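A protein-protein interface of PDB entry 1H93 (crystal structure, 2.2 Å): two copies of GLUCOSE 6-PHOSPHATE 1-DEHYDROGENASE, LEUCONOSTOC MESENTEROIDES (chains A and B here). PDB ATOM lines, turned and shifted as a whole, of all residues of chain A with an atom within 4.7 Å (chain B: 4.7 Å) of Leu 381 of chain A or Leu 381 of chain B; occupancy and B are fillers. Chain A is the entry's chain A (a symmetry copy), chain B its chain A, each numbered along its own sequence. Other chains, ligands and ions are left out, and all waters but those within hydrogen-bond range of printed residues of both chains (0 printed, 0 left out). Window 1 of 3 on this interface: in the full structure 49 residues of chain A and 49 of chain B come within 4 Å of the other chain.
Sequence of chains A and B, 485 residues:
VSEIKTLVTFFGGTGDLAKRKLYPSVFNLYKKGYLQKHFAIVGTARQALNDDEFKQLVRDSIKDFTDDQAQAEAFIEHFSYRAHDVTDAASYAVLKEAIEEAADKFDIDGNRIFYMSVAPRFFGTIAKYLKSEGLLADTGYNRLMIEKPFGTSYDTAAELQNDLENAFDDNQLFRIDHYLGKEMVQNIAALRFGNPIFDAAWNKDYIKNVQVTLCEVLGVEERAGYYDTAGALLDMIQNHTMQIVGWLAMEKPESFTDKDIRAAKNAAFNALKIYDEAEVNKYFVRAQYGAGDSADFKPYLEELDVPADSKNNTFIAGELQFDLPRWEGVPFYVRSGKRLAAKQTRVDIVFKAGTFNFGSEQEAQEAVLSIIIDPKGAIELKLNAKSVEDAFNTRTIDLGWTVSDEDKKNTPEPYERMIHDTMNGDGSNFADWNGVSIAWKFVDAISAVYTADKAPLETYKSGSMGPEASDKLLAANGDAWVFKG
O of Leu 399 of chain B sits at hydrogen-bond distance from N of Leu 381 of chain B (2.8 Å).
O of Leu 383 of chain B sits at hydrogen-bond distance from N of Ile 397 of chain B (2.9 Å).
The backbone carbonyl oxygen (O) of Leu 399 of chain A is in hydrogen-bond range of the backbone NH (N) of Leu 381 of chain A (2.8 Å).
The backbone carbonyl oxygen of Leu 383 of chain A is in hydrogen-bond range of the backbone NH of Ile 397 of chain A, 2.9 Å away.
Among the printed residues, merely in contact across the chains: Phe 198 of chain A with Leu 383 of chain B (3.6 Å), Ile 379 of chain A with Ile 397 of chain B (3.5 Å), Ile 379 of chain A with Leu 399 of chain B (3.2 Å), Leu 381 of chain A with Leu 381 of chain B (3.2 Å), Leu 383 of chain A with Phe 198 of chain B (3.6 Å), Ile 397 of chain A with Ile 379 of chain B (3.5 Å), Leu 399 of chain A with Ile 379 of chain B (3.2 Å) and Leu 399 of chain A with Leu 399 of chain B (3.8 Å).
Leu 381 of chain A touches one residue of chain B.
Leu 381 of chain B touches one residue of chain A.
Of the printed residues of chain A, Leu 399 of chain B touches Ile 379 (3.2 Å) and Leu 399 (3.8 Å).
Printed residues of chain B within 4 Å of Leu 383 of chain A: Phe 198.
Printed residues of chain B within 4 Å of Ile 397 of chain A: Ile 379 (3.5 Å).
Printed residues of chain B within 4 Å of Phe 198 of chain A: Leu 383 (3.6 Å).
Of the printed residues of chain A, Phe 198 of chain B touches Leu 383.
The nearest residue of chain A that does not touch Leu 381 of chain B is Leu 399 of chain A (4.3 Å).
The nearest printed residue of chain A that does not touch Leu 383 of chain B is Leu 381 of chain A (5.0 Å).
Of the 11 printed residues of chain A, 6 touch a printed residue of chain B.
Along chain B the printed residues that touch a printed residue of chain A span positions 198 to 399.
Among the printed residues, no Asp or Glu carboxylate lies within 4 Å of a Lys or Arg side-chain nitrogen of the other chain.
Phe 198 of chain A touches Leu 383 of chain B, and with the chains exchanged Leu 383 of chain A touches Phe 198 of chain B.
Ile 379 of chain A touches Ile 397 of chain B, and with the chains exchanged Ile 397 of chain A touches Ile 379 of chain B.
Leu 381 of chain A touches its own counterpart, Leu 381 of chain B.
Leu 399 of chain A touches its own counterpart, Leu 399 of chain B.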
ATOM      1  N   PHE A 198     -11.557  -3.447   7.781  1.00  0.00           N
ATOM      2  CA  PHE A 198     -10.453  -3.184   6.864  1.00  0.00           C
ATOM      3  C   PHE A 198     -10.938  -2.251   5.759  1.00  0.00           C
ATOM      4  O   PHE A 198     -10.267  -1.290   5.404  1.00  0.00           O
ATOM      5  CB  PHE A 198      -9.901  -4.487   6.287  1.00  0.00           C
ATOM      6  CG  PHE A 198      -9.057  -5.272   7.257  1.00  0.00           C
ATOM      7  CD1 PHE A 198      -8.056  -4.647   7.997  1.00  0.00           C
ATOM      8  CD2 PHE A 198      -9.243  -6.640   7.409  1.00  0.00           C
ATOM      9  CE1 PHE A 198      -7.252  -5.374   8.871  1.00  0.00           C
ATOM     10  CE2 PHE A 198      -8.445  -7.373   8.278  1.00  0.00           C
ATOM     11  CZ  PHE A 198      -7.446  -6.739   9.010  1.00  0.00           C
ATOM     12  N   VAL A 368       0.356  -4.102  11.211  1.00  0.00           N
ATOM     13  CA  VAL A 368       0.714  -4.499   9.851  1.00  0.00           C
ATOM     14  C   VAL A 368      -0.091  -5.693   9.354  1.00  0.00           C
ATOM     15  O   VAL A 368      -0.166  -6.720  10.031  1.00  0.00           O
ATOM     16  CB  VAL A 368       2.224  -4.864   9.756  1.00  0.00           C
ATOM     17  CG1 VAL A 368       2.583  -5.294   8.342  1.00  0.00           C
ATOM     18  CG2 VAL A 368       3.094  -3.691  10.195  1.00  0.00           C
ATOM     19  N   LEU A 369      -0.732  -5.533   8.199  1.00  0.00           N
ATOM     20  CA  LEU A 369      -1.493  -6.615   7.579  1.00  0.00           C
ATOM     21  C   LEU A 369      -0.627  -7.120   6.421  1.00  0.00           C
ATOM     22  O   LEU A 369      -0.378  -6.390   5.457  1.00  0.00           O
ATOM     23  CB  LEU A 369      -2.837  -6.118   7.048  1.00  0.00           C
ATOM     24  CG  LEU A 369      -3.622  -7.121   6.194  1.00  0.00           C
ATOM     25  CD1 LEU A 369      -3.973  -8.361   7.000  1.00  0.00           C
ATOM     26  CD2 LEU A 369      -4.878  -6.471   5.644  1.00  0.00           C
ATOM     27  N   ILE A 379      -1.483 -15.242   5.799  1.00  0.00           N
ATOM     28  CA  ILE A 379      -1.958 -13.909   6.148  1.00  0.00           C
ATOM     29  C   ILE A 379      -1.535 -13.662   7.591  1.00  0.00           C
ATOM     30  O   ILE A 379      -1.742 -14.512   8.460  1.00  0.00           O
ATOM     31  CB  ILE A 379      -3.501 -13.809   6.033  1.00  0.00           C
ATOM     32  CG1 ILE A 379      -3.950 -14.132   4.603  1.00  0.00           C
ATOM     33  CG2 ILE A 379      -3.976 -12.416   6.431  1.00  0.00           C
ATOM     34  CD1 ILE A 379      -5.447 -14.227   4.426  1.00  0.00           C
ATOM     35  N   GLU A 380      -0.869 -12.542   7.832  1.00  0.00           N
ATOM     36  CA  GLU A 380      -0.427 -12.205   9.173  1.00  0.00           C
ATOM     37  C   GLU A 380      -0.934 -10.819   9.550  1.00  0.00           C
ATOM     38  O   GLU A 380      -1.037  -9.933   8.697  1.00  0.00           O
ATOM     39  CB  GLU A 380       1.104 -12.255   9.276  1.00  0.00           C
ATOM     40  CG  GLU A 380       1.631 -11.876  10.662  1.00  0.00           C
ATOM     41  CD  GLU A 380       3.147 -11.884  10.763  1.00  0.00           C
ATOM     42  OE1 GLU A 380       3.726 -12.976  10.961  1.00  0.00           O
ATOM     43  OE2 GLU A 380       3.758 -10.793  10.674  1.00  0.00           O
ATOM     44  N   LEU A 381      -1.314 -10.658  10.813  1.00  0.00           N
ATOM     45  CA  LEU A 381      -1.786  -9.375  11.314  1.00  0.00           C
ATOM     46  C   LEU A 381      -1.034  -9.057  12.596  1.00  0.00           C
ATOM     47  O   LEU A 381      -1.191  -9.745  13.605  1.00  0.00           O
ATOM     48  CB  LEU A 381      -3.294  -9.396  11.575  1.00  0.00           C
ATOM     49  CG  LEU A 381      -3.905  -8.068  12.039  1.00  0.00           C
ATOM     50  CD1 LEU A 381      -3.596  -6.943  11.075  1.00  0.00           C
ATOM     51  CD2 LEU A 381      -5.391  -8.230  12.168  1.00  0.00           C
ATOM     52  N   LYS A 382      -0.142  -8.079  12.508  1.00  0.00           N
ATOM     53  CA  LYS A 382       0.656  -7.640  13.637  1.00  0.00           C
ATOM     54  C   LYS A 382      -0.162  -6.578  14.359  1.00  0.00           C
ATOM     55  O   LYS A 382      -0.551  -5.574  13.754  1.00  0.00           O
ATOM     56  CB  LYS A 382       1.980  -7.046  13.150  1.00  0.00           C
ATOM     57  CG  LYS A 382       2.924  -6.621  14.261  1.00  0.00           C
ATOM     58  CD  LYS A 382       4.109  -5.841  13.717  1.00  0.00           C
ATOM     59  CE  LYS A 382       5.328  -6.723  13.451  1.00  0.00           C
ATOM     60  NZ  LYS A 382       5.086  -7.840  12.499  1.00  0.00           N
ATOM     61  N   LEU A 383      -0.428  -6.812  15.642  1.00  0.00           N
ATOM     62  CA  LEU A 383      -1.219  -5.894  16.456  1.00  0.00           C
ATOM     63  C   LEU A 383      -0.511  -5.466  17.736  1.00  0.00           C
ATOM     64  O   LEU A 383       0.456  -6.095  18.178  1.00  0.00           O
ATOM     65  CB  LEU A 383      -2.554  -6.545  16.829  1.00  0.00           C
ATOM     66  CG  LEU A 383      -3.553  -6.818  15.702  1.00  0.00           C
ATOM     67  CD1 LEU A 383      -4.636  -7.775  16.178  1.00  0.00           C
ATOM     68  CD2 LEU A 383      -4.152  -5.511  15.211  1.00  0.00           C
ATOM     69  N   ILE A 397       2.362  -8.189  18.591  1.00  0.00           N
ATOM     70  CA  ILE A 397       2.239  -9.640  18.550  1.00  0.00           C
ATOM     71  C   ILE A 397       1.766  -9.993  17.142  1.00  0.00           C
ATOM     72  O   ILE A 397       1.140  -9.166  16.466  1.00  0.00           O
ATOM     73  CB  ILE A 397       1.221 -10.159  19.595  1.00  0.00           C
ATOM     74  CG1 ILE A 397      -0.123  -9.446  19.427  1.00  0.00           C
ATOM     75  CG2 ILE A 397       1.774  -9.960  21.001  1.00  0.00           C
ATOM     76  CD1 ILE A 397      -1.273 -10.143  20.097  1.00  0.00           C
ATOM     77  N   ASP A 398       2.023 -11.221  16.710  1.00  0.00           N
ATOM     78  CA  ASP A 398       1.643 -11.622  15.365  1.00  0.00           C
ATOM     79  C   ASP A 398       0.577 -12.696  15.299  1.00  0.00           C
ATOM     80  O   ASP A 398       0.771 -13.798  15.798  1.00  0.00           O
ATOM     81  CB  ASP A 398       2.880 -12.078  14.583  1.00  0.00           C
ATOM     82  CG  ASP A 398       3.945 -10.995  14.485  1.00  0.00           C
ATOM     83  OD1 ASP A 398       3.619  -9.862  14.074  1.00  0.00           O
ATOM     84  OD2 ASP A 398       5.115 -11.274  14.816  1.00  0.00           O
ATOM     85  N   LEU A 399      -0.559 -12.347  14.703  1.00  0.00           N
ATOM     86  CA  LEU A 399      -1.672 -13.269  14.502  1.00  0.00           C
ATOM     87  C   LEU A 399      -1.400 -13.862  13.122  1.00  0.00           C
ATOM     88  O   LEU A 399      -1.094 -13.121  12.186  1.00  0.00           O
ATOM     89  CB  LEU A 399      -2.996 -12.499  14.449  1.00  0.00           C
ATOM     90  CG  LEU A 399      -3.698 -11.927  15.688  1.00  0.00           C
ATOM     91  CD1 LEU A 399      -4.521 -13.002  16.336  1.00  0.00           C
ATOM     92  CD2 LEU A 399      -2.707 -11.312  16.672  1.00  0.00           C
ATOM     93  N   PHE B 198      -9.126  -1.014  15.487  1.00  0.00           N
ATOM     94  CA  PHE B 198     -10.075  -1.569  16.447  1.00  0.00           C
ATOM     95  C   PHE B 198     -10.696  -0.428  17.246  1.00  0.00           C
ATOM     96  O   PHE B 198     -11.902  -0.386  17.453  1.00  0.00           O
ATOM     97  CB  PHE B 198      -9.391  -2.581  17.365  1.00  0.00           C
ATOM     98  CG  PHE B 198      -9.109  -3.906  16.706  1.00  0.00           C
ATOM     99  CD1 PHE B 198     -10.095  -4.559  15.970  1.00  0.00           C
ATOM    100  CD2 PHE B 198      -7.868  -4.515  16.846  1.00  0.00           C
ATOM    101  CE1 PHE B 198      -9.849  -5.799  15.387  1.00  0.00           C
ATOM    102  CE2 PHE B 198      -7.615  -5.752  16.268  1.00  0.00           C
ATOM    103  CZ  PHE B 198      -8.608  -6.397  15.536  1.00  0.00           C
ATOM    104  N   VAL B 368     -14.898 -11.867  13.754  1.00  0.00           N
ATOM    105  CA  VAL B 368     -14.940 -12.063  15.201  1.00  0.00           C
ATOM    106  C   VAL B 368     -13.570 -11.927  15.854  1.00  0.00           C
ATOM    107  O   VAL B 368     -12.607 -12.564  15.422  1.00  0.00           O
ATOM    108  CB  VAL B 368     -15.505 -13.469  15.557  1.00  0.00           C
ATOM    109  CG1 VAL B 368     -15.526 -13.672  17.064  1.00  0.00           C
ATOM    110  CG2 VAL B 368     -16.901 -13.656  14.972  1.00  0.00           C
ATOM    111  N   LEU B 369     -13.478 -11.058  16.858  1.00  0.00           N
ATOM    112  CA  LEU B 369     -12.240 -10.871  17.609  1.00  0.00           C
ATOM    113  C   LEU B 369     -12.455 -11.585  18.947  1.00  0.00           C
ATOM    114  O   LEU B 369     -13.308 -11.183  19.744  1.00  0.00           O
ATOM    115  CB  LEU B 369     -11.952  -9.389  17.848  1.00  0.00           C
ATOM    116  CG  LEU B 369     -10.792  -9.088  18.806  1.00  0.00           C
ATOM    117  CD1 LEU B 369      -9.484  -9.641  18.264  1.00  0.00           C
ATOM    118  CD2 LEU B 369     -10.681  -7.593  19.039  1.00  0.00           C
ATOM    119  N   ILE B 379      -5.413 -15.057  21.278  1.00  0.00           N
ATOM    120  CA  ILE B 379      -6.192 -14.040  20.583  1.00  0.00           C
ATOM    121  C   ILE B 379      -6.458 -14.580  19.183  1.00  0.00           C
ATOM    122  O   ILE B 379      -5.542 -15.058  18.510  1.00  0.00           O
ATOM    123  CB  ILE B 379      -5.416 -12.700  20.485  1.00  0.00           C
ATOM    124  CG1 ILE B 379      -5.072 -12.183  21.887  1.00  0.00           C
ATOM    125  CG2 ILE B 379      -6.239 -11.663  19.729  1.00  0.00           C
ATOM    126  CD1 ILE B 379      -4.171 -10.970  21.899  1.00  0.00           C
ATOM    127  N   GLU B 380      -7.720 -14.584  18.777  1.00  0.00           N
ATOM    128  CA  GLU B 380      -8.082 -15.069  17.458  1.00  0.00           C
ATOM    129  C   GLU B 380      -8.884 -14.004  16.719  1.00  0.00           C
ATOM    130  O   GLU B 380      -9.652 -13.257  17.332  1.00  0.00           O
ATOM    131  CB  GLU B 380      -8.893 -16.369  17.554  1.00  0.00           C
ATOM    132  CG  GLU B 380      -9.333 -16.911  16.192  1.00  0.00           C
ATOM    133  CD  GLU B 380     -10.170 -18.177  16.279  1.00  0.00           C
ATOM    134  OE1 GLU B 380      -9.580 -19.274  16.404  1.00  0.00           O
ATOM    135  OE2 GLU B 380     -11.416 -18.077  16.192  1.00  0.00           O
ATOM    136  N   LEU B 381      -8.648 -13.893  15.416  1.00  0.00           N
ATOM    137  CA  LEU B 381      -9.370 -12.940  14.586  1.00  0.00           C
ATOM    138  C   LEU B 381      -9.900 -13.675  13.366  1.00  0.00           C
ATOM    139  O   LEU B 381      -9.128 -14.140  12.526  1.00  0.00           O
ATOM    140  CB  LEU B 381      -8.471 -11.778  14.157  1.00  0.00           C
ATOM    141  CG  LEU B 381      -9.155 -10.678  13.334  1.00  0.00           C
ATOM    142  CD1 LEU B 381     -10.365 -10.116  14.050  1.00  0.00           C
ATOM    143  CD2 LEU B 381      -8.169  -9.580  13.068  1.00  0.00           C
ATOM    144  N   LYS B 382     -11.213 -13.864  13.337  1.00  0.00           N
ATOM    145  CA  LYS B 382     -11.886 -14.538  12.242  1.00  0.00           C
ATOM    146  C   LYS B 382     -12.204 -13.468  11.206  1.00  0.00           C
ATOM    147  O   LYS B 382     -12.878 -12.481  11.518  1.00  0.00           O
ATOM    148  CB  LYS B 382     -13.176 -15.194  12.739  1.00  0.00           C
ATOM    149  CG  LYS B 382     -13.922 -15.990  11.683  1.00  0.00           C
ATOM    150  CD  LYS B 382     -15.293 -16.422  12.175  1.00  0.00           C
ATOM    151  CE  LYS B 382     -15.292 -17.825  12.778  1.00  0.00           C
ATOM    152  NZ  LYS B 382     -14.358 -18.006  13.921  1.00  0.00           N
ATOM    153  N   LEU B 383     -11.708 -13.666   9.987  1.00  0.00           N
ATOM    154  CA  LEU B 383     -11.914 -12.715   8.898  1.00  0.00           C
ATOM    155  C   LEU B 383     -12.510 -13.355   7.649  1.00  0.00           C
ATOM    156  O   LEU B 383     -12.488 -14.579   7.480  1.00  0.00           O
ATOM    157  CB  LEU B 383     -10.585 -12.054   8.523  1.00  0.00           C
ATOM    158  CG  LEU B 383      -9.934 -11.129   9.554  1.00  0.00           C
ATOM    159  CD1 LEU B 383      -8.484 -10.860   9.180  1.00  0.00           C
ATOM    160  CD2 LEU B 383     -10.723  -9.835   9.662  1.00  0.00           C
ATOM    161  N   ILE B 397     -11.802 -17.340   7.783  1.00  0.00           N
ATOM    162  CA  ILE B 397     -10.553 -18.001   8.136  1.00  0.00           C
ATOM    163  C   ILE B 397     -10.167 -17.484   9.519  1.00  0.00           C
ATOM    164  O   ILE B 397     -10.571 -16.381   9.911  1.00  0.00           O
ATOM    165  CB  ILE B 397      -9.429 -17.681   7.120  1.00  0.00           C
ATOM    166  CG1 ILE B 397      -9.273 -16.167   6.959  1.00  0.00           C
ATOM    167  CG2 ILE B 397      -9.734 -18.344   5.782  1.00  0.00           C
ATOM    168  CD1 ILE B 397      -7.974 -15.748   6.330  1.00  0.00           C
ATOM    169  N   ASP B 398      -9.361 -18.249  10.245  1.00  0.00           N
ATOM    170  CA  ASP B 398      -8.981 -17.848  11.589  1.00  0.00           C
ATOM    171  C   ASP B 398      -7.511 -17.532  11.767  1.00  0.00           C
ATOM    172  O   ASP B 398      -6.660 -18.388  11.557  1.00  0.00           O
ATOM    173  CB  ASP B 398      -9.401 -18.924  12.597  1.00  0.00           C
ATOM    174  CG  ASP B 398     -10.898 -19.196  12.576  1.00  0.00           C
ATOM    175  OD1 ASP B 398     -11.689 -18.236  12.678  1.00  0.00           O
ATOM    176  OD2 ASP B 398     -11.290 -20.375  12.460  1.00  0.00           O
ATOM    177  N   LEU B 399      -7.226 -16.285  12.128  1.00  0.00           N
ATOM    178  CA  LEU B 399      -5.870 -15.820  12.396  1.00  0.00           C
ATOM    179  C   LEU B 399      -5.705 -16.045  13.897  1.00  0.00           C
ATOM    180  O   LEU B 399      -6.595 -15.690  14.671  1.00  0.00           O
ATOM    181  CB  LEU B 399      -5.758 -14.317  12.115  1.00  0.00           C
ATOM    182  CG  LEU B 399      -5.680 -13.720  10.703  1.00  0.00           C
ATOM    183  CD1 LEU B 399      -4.260 -13.764  10.220  1.00  0.00           C
ATOM    184  CD2 LEU B 399      -6.623 -14.424   9.733  1.00  0.00           C
